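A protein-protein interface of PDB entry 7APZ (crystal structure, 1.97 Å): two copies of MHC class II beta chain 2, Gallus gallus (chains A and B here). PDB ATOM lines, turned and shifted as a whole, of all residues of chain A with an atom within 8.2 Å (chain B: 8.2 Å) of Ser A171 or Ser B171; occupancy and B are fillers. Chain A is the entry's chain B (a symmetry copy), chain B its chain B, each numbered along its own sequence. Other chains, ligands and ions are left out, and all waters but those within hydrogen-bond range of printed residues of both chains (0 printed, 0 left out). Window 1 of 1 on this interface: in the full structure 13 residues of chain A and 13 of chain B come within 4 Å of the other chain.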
ATOM      1  N   CYS A 144      17.704 -33.503  29.669  1.00  0.00           N
ATOM      2  CA  CYS A 144      16.601 -34.235  29.000  1.00  0.00           C
ATOM      3  C   CYS A 144      16.880 -34.178  27.507  1.00  0.00           C
ATOM      4  O   CYS A 144      16.766 -33.074  26.906  1.00  0.00           O
ATOM      5  CB  CYS A 144      15.246 -33.661  29.322  1.00  0.00           C
ATOM      6  SG  CYS A 144      13.932 -34.770  28.756  1.00  0.00           S
ATOM      7  N   ILE A 154       7.544 -29.364  19.646  1.00  0.00           N
ATOM      8  CA  ILE A 154       7.630 -30.303  20.795  1.00  0.00           C
ATOM      9  C   ILE A 154       7.625 -29.468  22.075  1.00  0.00           C
ATOM     10  O   ILE A 154       8.073 -28.321  22.010  1.00  0.00           O
ATOM     11  CB  ILE A 154       8.875 -31.197  20.639  1.00  0.00           C
ATOM     12  CG1 ILE A 154       8.805 -32.409  21.569  1.00  0.00           C
ATOM     13  CG2 ILE A 154      10.165 -30.385  20.785  1.00  0.00           C
ATOM     14  CD1 ILE A 154       9.869 -33.474  21.318  1.00  0.00           C
ATOM     15  N   VAL A 156       9.037 -29.774  26.014  1.00  0.00           N
ATOM     16  CA  VAL A 156       9.969 -30.537  26.880  1.00  0.00           C
ATOM     17  C   VAL A 156      10.144 -29.692  28.142  1.00  0.00           C
ATOM     18  O   VAL A 156      10.683 -28.587  28.006  1.00  0.00           O
ATOM     19  CB  VAL A 156      11.287 -30.827  26.149  1.00  0.00           C
ATOM     20  CG1 VAL A 156      12.235 -31.642  27.021  1.00  0.00           C
ATOM     21  CG2 VAL A 156      11.034 -31.581  24.846  1.00  0.00           C
ATOM     22  N   ARG A 168      16.462 -21.620  35.786  1.00  0.00           N
ATOM     23  CA  ARG A 168      17.696 -22.418  35.571  1.00  0.00           C
ATOM     24  C   ARG A 168      17.382 -23.575  34.609  1.00  0.00           C
ATOM     25  O   ARG A 168      18.061 -24.622  34.731  1.00  0.00           O
ATOM     26  CB  ARG A 168      18.243 -22.909  36.919  1.00  0.00           C
ATOM     27  CG  ARG A 168      18.249 -21.857  38.024  1.00  0.00           C
ATOM     28  CD  ARG A 168      19.190 -22.175  39.177  1.00  0.00           C
ATOM     29  NE  ARG A 168      20.585 -21.982  38.795  1.00  0.00           N
ATOM     30  CZ  ARG A 168      21.638 -22.589  39.355  1.00  0.00           C
ATOM     31  NH1 ARG A 168      22.854 -22.343  38.897  1.00  0.00           N
ATOM     32  NH2 ARG A 168      21.479 -23.448  40.351  1.00  0.00           N
ATOM     33  N   VAL A 169      16.388 -23.409  33.715  1.00  0.00           N
ATOM     34  CA  VAL A 169      16.157 -24.312  32.544  1.00  0.00           C
ATOM     35  C   VAL A 169      16.736 -23.663  31.293  1.00  0.00           C
ATOM     36  O   VAL A 169      16.316 -22.549  30.954  1.00  0.00           O
ATOM     37  CB  VAL A 169      14.685 -24.673  32.293  1.00  0.00           C
ATOM     38  CG1 VAL A 169      14.553 -25.500  31.013  1.00  0.00           C
ATOM     39  CG2 VAL A 169      14.090 -25.406  33.479  1.00  0.00           C
ATOM     40  N   VAL A 170      17.674 -24.368  30.665  1.00  0.00           N
ATOM     41  CA  VAL A 170      18.323 -23.904  29.414  1.00  0.00           C
ATOM     42  C   VAL A 170      17.944 -24.909  28.317  1.00  0.00           C
ATOM     43  O   VAL A 170      18.206 -26.104  28.497  1.00  0.00           O
ATOM     44  CB  VAL A 170      19.850 -23.846  29.598  1.00  0.00           C
ATOM     45  CG1 VAL A 170      20.605 -24.041  28.295  1.00  0.00           C
ATOM     46  CG2 VAL A 170      20.280 -22.561  30.282  1.00  0.00           C
ATOM     47  N   SER A 171      17.326 -24.431  27.241  1.00  0.00           N
ATOM     48  CA  SER A 171      16.936 -25.308  26.113  1.00  0.00           C
ATOM     49  C   SER A 171      17.688 -24.923  24.850  1.00  0.00           C
ATOM     50  O   SER A 171      17.690 -23.735  24.515  1.00  0.00           O
ATOM     51  CB  SER A 171      15.476 -25.251  25.860  1.00  0.00           C
ATOM     52  OG  SER A 171      15.143 -25.985  24.694  1.00  0.00           O
ATOM     53  N   THR A 172      18.287 -25.898  24.181  1.00  0.00           N
ATOM     54  CA  THR A 172      18.904 -25.633  22.865  1.00  0.00           C
ATOM     55  C   THR A 172      17.750 -25.427  21.893  1.00  0.00           C
ATOM     56  O   THR A 172      16.605 -25.675  22.258  1.00  0.00           O
ATOM     57  CB  THR A 172      19.658 -26.854  22.317  1.00  0.00           C
ATOM     58  OG1 THR A 172      18.737 -27.910  22.046  1.00  0.00           O
ATOM     59  CG2 THR A 172      20.755 -27.339  23.236  1.00  0.00           C
ATOM     60  N   ASP A 173      18.044 -24.938  20.706  1.00  0.00           N
ATOM     61  CA  ASP A 173      16.962 -24.859  19.701  1.00  0.00           C
ATOM     62  C   ASP A 173      16.631 -26.282  19.253  1.00  0.00           C
ATOM     63  O   ASP A 173      17.472 -27.166  19.446  1.00  0.00           O
ATOM     64  CB  ASP A 173      17.383 -24.035  18.488  1.00  0.00           C
ATOM     65  CG  ASP A 173      16.250 -23.256  17.850  1.00  0.00           C
ATOM     66  OD1 ASP A 173      15.080 -23.571  18.131  1.00  0.00           O
ATOM     67  OD2 ASP A 173      16.552 -22.340  17.072  1.00  0.00           O
ATOM     68  N   VAL A 174      15.425 -26.495  18.733  1.00  0.00           N
ATOM     69  CA  VAL A 174      15.149 -27.819  18.130  1.00  0.00           C
ATOM     70  C   VAL A 174      16.134 -27.890  16.969  1.00  0.00           C
ATOM     71  O   VAL A 174      16.091 -27.010  16.118  1.00  0.00           O
ATOM     72  CB  VAL A 174      13.689 -27.953  17.668  1.00  0.00           C
ATOM     73  CG1 VAL A 174      13.424 -29.303  17.030  1.00  0.00           C
ATOM     74  CG2 VAL A 174      12.719 -27.698  18.810  1.00  0.00           C
ATOM     75  N   GLN A 183      16.033 -33.007  17.014  1.00  0.00           N
ATOM     76  CA  GLN A 183      16.500 -33.307  18.389  1.00  0.00           C
ATOM     77  C   GLN A 183      16.574 -32.019  19.207  1.00  0.00           C
ATOM     78  O   GLN A 183      16.729 -30.907  18.642  1.00  0.00           O
ATOM     79  CB  GLN A 183      17.845 -34.038  18.369  1.00  0.00           C
ATOM     80  CG  GLN A 183      18.995 -33.232  17.826  1.00  0.00           C
ATOM     81  CD  GLN A 183      20.286 -33.981  18.042  1.00  0.00           C
ATOM     82  OE1 GLN A 183      20.833 -33.991  19.148  1.00  0.00           O
ATOM     83  NE2 GLN A 183      20.787 -34.626  16.995  1.00  0.00           N
ATOM     84  N   VAL A 184      16.477 -32.168  20.515  1.00  0.00           N
ATOM     85  CA  VAL A 184      16.574 -31.005  21.437  1.00  0.00           C
ATOM     86  C   VAL A 184      17.114 -31.502  22.779  1.00  0.00           C
ATOM     87  O   VAL A 184      16.911 -32.711  23.098  1.00  0.00           O
ATOM     88  CB  VAL A 184      15.199 -30.323  21.547  1.00  0.00           C
ATOM     89  CG1 VAL A 184      14.169 -31.271  22.136  1.00  0.00           C
ATOM     90  CG2 VAL A 184      15.276 -29.024  22.352  1.00  0.00           C
ATOM     91  N   LEU A 185      17.777 -30.605  23.506  1.00  0.00           N
ATOM     92  CA  LEU A 185      18.419 -30.819  24.825  1.00  0.00           C
ATOM     93  C   LEU A 185      17.912 -29.733  25.776  1.00  0.00           C
ATOM     94  O   LEU A 185      17.983 -28.553  25.437  1.00  0.00           O
ATOM     95  CB  LEU A 185      19.943 -30.790  24.646  1.00  0.00           C
ATOM     96  CG  LEU A 185      20.777 -31.016  25.916  1.00  0.00           C
ATOM     97  CD1 LEU A 185      20.408 -32.314  26.590  1.00  0.00           C
ATOM     98  CD2 LEU A 185      22.264 -30.999  25.617  1.00  0.00           C
ATOM     99  N   VAL A 186      17.281 -30.140  26.874  1.00  0.00           N
ATOM    100  CA  VAL A 186      16.773 -29.222  27.929  1.00  0.00           C
ATOM    101  C   VAL A 186      17.453 -29.596  29.256  1.00  0.00           C
ATOM    102  O   VAL A 186      17.343 -30.740  29.677  1.00  0.00           O
ATOM    103  CB  VAL A 186      15.237 -29.260  27.985  1.00  0.00           C
ATOM    104  CG1 VAL A 186      14.674 -28.239  28.970  1.00  0.00           C
ATOM    105  CG2 VAL A 186      14.659 -29.035  26.605  1.00  0.00           C
ATOM    106  N   VAL A 187      18.247 -28.683  29.813  1.00  0.00           N
ATOM    107  CA  VAL A 187      19.076 -28.911  31.023  1.00  0.00           C
ATOM    108  C   VAL A 187      18.530 -28.066  32.174  1.00  0.00           C
ATOM    109  O   VAL A 187      18.252 -26.886  31.993  1.00  0.00           O
ATOM    110  CB  VAL A 187      20.555 -28.593  30.778  1.00  0.00           C
ATOM    111  CG1 VAL A 187      21.365 -28.833  32.038  1.00  0.00           C
ATOM    112  CG2 VAL A 187      21.118 -29.409  29.625  1.00  0.00           C
ATOM    113  N   LEU A 188      18.270 -28.701  33.302  1.00  0.00           N
ATOM    114  CA  LEU A 188      17.827 -28.021  34.536  1.00  0.00           C
ATOM    115  C   LEU A 188      19.051 -28.018  35.453  1.00  0.00           C
ATOM    116  O   LEU A 188      19.604 -29.090  35.663  1.00  0.00           O
ATOM    117  CB  LEU A 188      16.636 -28.767  35.143  1.00  0.00           C
ATOM    118  CG  LEU A 188      16.260 -28.355  36.568  1.00  0.00           C
ATOM    119  CD1 LEU A 188      15.795 -26.911  36.633  1.00  0.00           C
ATOM    120  CD2 LEU A 188      15.204 -29.270  37.120  1.00  0.00           C
ATOM    121  N   CYS B 144      17.939 -11.511  22.702  1.00  0.00           N
ATOM    122  CA  CYS B 144      18.240 -10.618  23.848  1.00  0.00           C
ATOM    123  C   CYS B 144      19.621 -11.006  24.354  1.00  0.00           C
ATOM    124  O   CYS B 144      19.768 -12.117  24.934  1.00  0.00           O
ATOM    125  CB  CYS B 144      17.212 -10.718  24.945  1.00  0.00           C
ATOM    126  SG  CYS B 144      17.441  -9.392  26.157  1.00  0.00           S
ATOM    127  N   ILE B 154      20.900 -14.215  37.010  1.00  0.00           N
ATOM    128  CA  ILE B 154      20.224 -13.158  36.212  1.00  0.00           C
ATOM    129  C   ILE B 154      18.890 -13.726  35.729  1.00  0.00           C
ATOM    130  O   ILE B 154      18.812 -14.947  35.574  1.00  0.00           O
ATOM    131  CB  ILE B 154      21.154 -12.698  35.074  1.00  0.00           C
ATOM    132  CG1 ILE B 154      20.676 -11.377  34.470  1.00  0.00           C
ATOM    133  CG2 ILE B 154      21.358 -13.808  34.038  1.00  0.00           C
ATOM    134  CD1 ILE B 154      21.657 -10.719  33.504  1.00  0.00           C
ATOM    135  N   VAL B 156      16.227 -13.171  32.535  1.00  0.00           N
ATOM    136  CA  VAL B 156      16.111 -12.571  31.183  1.00  0.00           C
ATOM    137  C   VAL B 156      14.868 -13.203  30.558  1.00  0.00           C
ATOM    138  O   VAL B 156      14.902 -14.422  30.352  1.00  0.00           O
ATOM    139  CB  VAL B 156      17.391 -12.798  30.368  1.00  0.00           C
ATOM    140  CG1 VAL B 156      17.292 -12.152  28.991  1.00  0.00           C
ATOM    141  CG2 VAL B 156      18.609 -12.236  31.097  1.00  0.00           C
ATOM    142  N   ARG B 168       8.778 -21.321  22.777  1.00  0.00           N
ATOM    143  CA  ARG B 168       9.726 -20.957  21.694  1.00  0.00           C
ATOM    144  C   ARG B 168      10.742 -19.940  22.238  1.00  0.00           C
ATOM    145  O   ARG B 168      11.232 -19.126  21.420  1.00  0.00           O
ATOM    146  CB  ARG B 168       8.953 -20.421  20.480  1.00  0.00           C
ATOM    147  CG  ARG B 168       7.711 -21.227  20.110  1.00  0.00           C
ATOM    148  CD  ARG B 168       7.226 -20.999  18.686  1.00  0.00           C
ATOM    149  NE  ARG B 168       8.104 -21.646  17.715  1.00  0.00           N
ATOM    150  CZ  ARG B 168       8.258 -21.279  16.437  1.00  0.00           C
ATOM    151  NH1 ARG B 168       9.106 -21.936  15.666  1.00  0.00           N
ATOM    152  NH2 ARG B 168       7.583 -20.253  15.938  1.00  0.00           N
ATOM    153  N   VAL B 169      11.026 -19.965  23.554  1.00  0.00           N
ATOM    154  CA  VAL B 169      12.184 -19.246  24.174  1.00  0.00           C
ATOM    155  C   VAL B 169      13.318 -20.237  24.405  1.00  0.00           C
ATOM    156  O   VAL B 169      13.107 -21.225  25.120  1.00  0.00           O
ATOM    157  CB  VAL B 169      11.861 -18.528  25.492  1.00  0.00           C
ATOM    158  CG1 VAL B 169      13.134 -17.927  26.094  1.00  0.00           C
ATOM    159  CG2 VAL B 169      10.800 -17.464  25.292  1.00  0.00           C
ATOM    160  N   VAL B 170      14.464 -19.947  23.792  1.00  0.00           N
ATOM    161  CA  VAL B 170      15.682 -20.783  23.932  1.00  0.00           C
ATOM    162  C   VAL B 170      16.742 -19.914  24.624  1.00  0.00           C
ATOM    163  O   VAL B 170      17.043 -18.831  24.108  1.00  0.00           O
ATOM    164  CB  VAL B 170      16.173 -21.243  22.548  1.00  0.00           C
ATOM    165  CG1 VAL B 170      17.669 -21.496  22.511  1.00  0.00           C
ATOM    166  CG2 VAL B 170      15.408 -22.461  22.063  1.00  0.00           C
ATOM    167  N   SER B 171      17.255 -20.371  25.762  1.00  0.00           N
ATOM    168  CA  SER B 171      18.299 -19.624  26.501  1.00  0.00           C
ATOM    169  C   SER B 171      19.595 -20.417  26.544  1.00  0.00           C
ATOM    170  O   SER B 171      19.542 -21.595  26.910  1.00  0.00           O
ATOM    171  CB  SER B 171      17.865 -19.303  27.881  1.00  0.00           C
ATOM    172  OG  SER B 171      18.926 -18.715  28.614  1.00  0.00           O
ATOM    173  N   THR B 172      20.705 -19.783  26.197  1.00  0.00           N
ATOM    174  CA  THR B 172      22.021 -20.433  26.362  1.00  0.00           C
ATOM    175  C   THR B 172      22.291 -20.463  27.860  1.00  0.00           C
ATOM    176  O   THR B 172      21.552 -19.840  28.616  1.00  0.00           O
ATOM    177  CB  THR B 172      23.166 -19.591  25.780  1.00  0.00           C
ATOM    178  OG1 THR B 172      23.299 -18.377  26.520  1.00  0.00           O
ATOM    179  CG2 THR B 172      22.997 -19.290  24.308  1.00  0.00           C
ATOM    180  N   ASP B 173      23.293 -21.210  28.275  1.00  0.00           N
ATOM    181  CA  ASP B 173      23.658 -21.146  29.708  1.00  0.00           C
ATOM    182  C   ASP B 173      24.304 -19.787  29.968  1.00  0.00           C
ATOM    183  O   ASP B 173      24.757 -19.160  29.005  1.00  0.00           O
ATOM    184  CB  ASP B 173      24.641 -22.250  30.085  1.00  0.00           C
ATOM    185  CG  ASP B 173      24.471 -22.769  31.499  1.00  0.00           C
ATOM    186  OD1 ASP B 173      23.813 -22.090  32.305  1.00  0.00           O
ATOM    187  OD2 ASP B 173      25.004 -23.851  31.779  1.00  0.00           O
ATOM    188  N   VAL B 174      24.284 -19.329  31.218  1.00  0.00           N
ATOM    189  CA  VAL B 174      25.058 -18.104  31.524  1.00  0.00           C
ATOM    190  C   VAL B 174      26.498 -18.517  31.241  1.00  0.00           C
ATOM    191  O   VAL B 174      26.954 -19.478  31.847  1.00  0.00           O
ATOM    192  CB  VAL B 174      24.856 -17.639  32.975  1.00  0.00           C
ATOM    193  CG1 VAL B 174      25.672 -16.399  33.286  1.00  0.00           C
ATOM    194  CG2 VAL B 174      23.386 -17.408  33.285  1.00  0.00           C
ATOM    195  N   GLN B 183      27.878 -13.654  30.436  1.00  0.00           N
ATOM    196  CA  GLN B 183      26.993 -13.271  29.309  1.00  0.00           C
ATOM    197  C   GLN B 183      25.959 -14.368  29.063  1.00  0.00           C
ATOM    198  O   GLN B 183      26.190 -15.556  29.398  1.00  0.00           O
ATOM    199  CB  GLN B 183      27.803 -12.969  28.047  1.00  0.00           C
ATOM    200  CG  GLN B 183      28.537 -14.151  27.468  1.00  0.00           C
ATOM    201  CD  GLN B 183      29.128 -13.776  26.132  1.00  0.00           C
ATOM    202  OE1 GLN B 183      28.423 -13.735  25.120  1.00  0.00           O
ATOM    203  NE2 GLN B 183      30.424 -13.489  26.109  1.00  0.00           N
ATOM    204  N   VAL B 184      24.842 -13.977  28.477  1.00  0.00           N
ATOM    205  CA  VAL B 184      23.763 -14.944  28.140  1.00  0.00           C
ATOM    206  C   VAL B 184      22.995 -14.401  26.933  1.00  0.00           C
ATOM    207  O   VAL B 184      22.979 -13.149  26.744  1.00  0.00           O
ATOM    208  CB  VAL B 184      22.877 -15.176  29.375  1.00  0.00           C
ATOM    209  CG1 VAL B 184      22.198 -13.886  29.805  1.00  0.00           C
ATOM    210  CG2 VAL B 184      21.852 -16.285  29.135  1.00  0.00           C
ATOM    211  N   LEU B 185      22.406 -15.313  26.163  1.00  0.00           N
ATOM    212  CA  LEU B 185      21.619 -15.070  24.929  1.00  0.00           C
ATOM    213  C   LEU B 185      20.277 -15.788  25.080  1.00  0.00           C
ATOM    214  O   LEU B 185      20.260 -16.979  25.386  1.00  0.00           O
ATOM    215  CB  LEU B 185      22.427 -15.564  23.722  1.00  0.00           C
ATOM    216  CG  LEU B 185      21.769 -15.372  22.346  1.00  0.00           C
ATOM    217  CD1 LEU B 185      21.404 -13.928  22.110  1.00  0.00           C
ATOM    218  CD2 LEU B 185      22.666 -15.864  21.226  1.00  0.00           C
ATOM    219  N   VAL B 186      19.181 -15.036  25.010  1.00  0.00           N
ATOM    220  CA  VAL B 186      17.797 -15.577  25.081  1.00  0.00           C
ATOM    221  C   VAL B 186      17.065 -15.194  23.785  1.00  0.00           C
ATOM    222  O   VAL B 186      16.986 -14.011  23.477  1.00  0.00           O
ATOM    223  CB  VAL B 186      17.091 -15.094  26.358  1.00  0.00           C
ATOM    224  CG1 VAL B 186      15.714 -15.728  26.529  1.00  0.00           C
ATOM    225  CG2 VAL B 186      17.955 -15.375  27.569  1.00  0.00           C
ATOM    226  N   VAL B 187      16.674 -16.187  22.988  1.00  0.00           N
ATOM    227  CA  VAL B 187      16.067 -16.003  21.646  1.00  0.00           C
ATOM    228  C   VAL B 187      14.604 -16.447  21.690  1.00  0.00           C
ATOM    229  O   VAL B 187      14.301 -17.512  22.217  1.00  0.00           O
ATOM    230  CB  VAL B 187      16.828 -16.767  20.557  1.00  0.00           C
ATOM    231  CG1 VAL B 187      16.172 -16.558  19.206  1.00  0.00           C
ATOM    232  CG2 VAL B 187      18.291 -16.355  20.505  1.00  0.00           C
ATOM    233  N   LEU B 188      13.710 -15.583  21.250  1.00  0.00           N
ATOM    234  CA  LEU B 188      12.269 -15.887  21.137  1.00  0.00           C
ATOM    235  C   LEU B 188      12.017 -16.084  19.641  1.00  0.00           C
ATOM    236  O   LEU B 188      12.385 -15.195  18.883  1.00  0.00           O
ATOM    237  CB  LEU B 188      11.446 -14.740  21.729  1.00  0.00           C
ATOM    238  CG  LEU B 188       9.948 -14.778  21.419  1.00  0.00           C
ATOM    239  CD1 LEU B 188       9.278 -15.996  22.030  1.00  0.00           C
ATOM    240  CD2 LEU B 188       9.278 -13.520  21.894  1.00  0.00           C
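O of Val A170 is in hydrogen-bond range of N of Val A187, at 2.9 Å.
The backbone carbonyl oxygen of Leu B185 sits at hydrogen-bond distance from the backbone NH of Thr B172.
The backbone carbonyl oxygen (O) of Val B170 sits at hydrogen-bond distance from the backbone NH (N) of Val B187.
N of Thr A172 lies within hydrogen-bond range of O of Leu A185 (3.0 Å).
Among the printed residues, merely in contact across the chains: Ser A171 with Val B170 (3.0 Å), Val A170 with Ser B171 (3.0 Å), Val A170 with Thr B172 (3.4 Å), Thr A172 with Val B170 (3.4 Å), Ser A171 with Ser B171 (3.6 Å), Val A170 with Asp B173 (3.7 Å) and Asp A173 with Val B170 (3.7 Å).
Ser A171 touches just these residues of chain B: Val B170 and Ser B171.
Printed residues of chain A within 4 Å of Ser B171: Val A170 (3.0 Å) and Ser A171 (3.6 Å).
Of chain B, only Ser B171, Thr B172 and Asp B173 come within 4 Å of Val A170.
Of the printed residues of chain B, Asp A173 touches Val B170 (3.7 Å).
Of the printed residues of chain A, Asp B173 touches Val A170 (3.7 Å).
Of the printed residues of chain B, Thr A172 touches Val B170.
Printed residues of chain A within 4 Å of Thr B172: Val A170 (3.4 Å).
Val A169 touches none of the printed residues of chain B.
Hydrophobic or aromatic side chains of chain B within 4 Å of the printed part of chain A: Val B170.
Of the 16 printed residues of chain A, 4 touch a printed residue of chain B.
Among the printed residues, 7 pairs touch across the chains.
Val A170 touches Ser B171, and with the chains exchanged Ser A171 touches Val B170.
Val A170 touches Thr B172, and with the chains exchanged Thr A172 touches Val B170.
Val A170 touches Asp B173, and with the chains exchanged Asp A173 touches Val B170.
Ser A171 touches its own counterpart, Ser B171.
Positions printed for both chains: 144, 154, 156, 168, 169, 170, 171, 172, 173, 174, 183, 184, 185, 186, 187 and 188.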
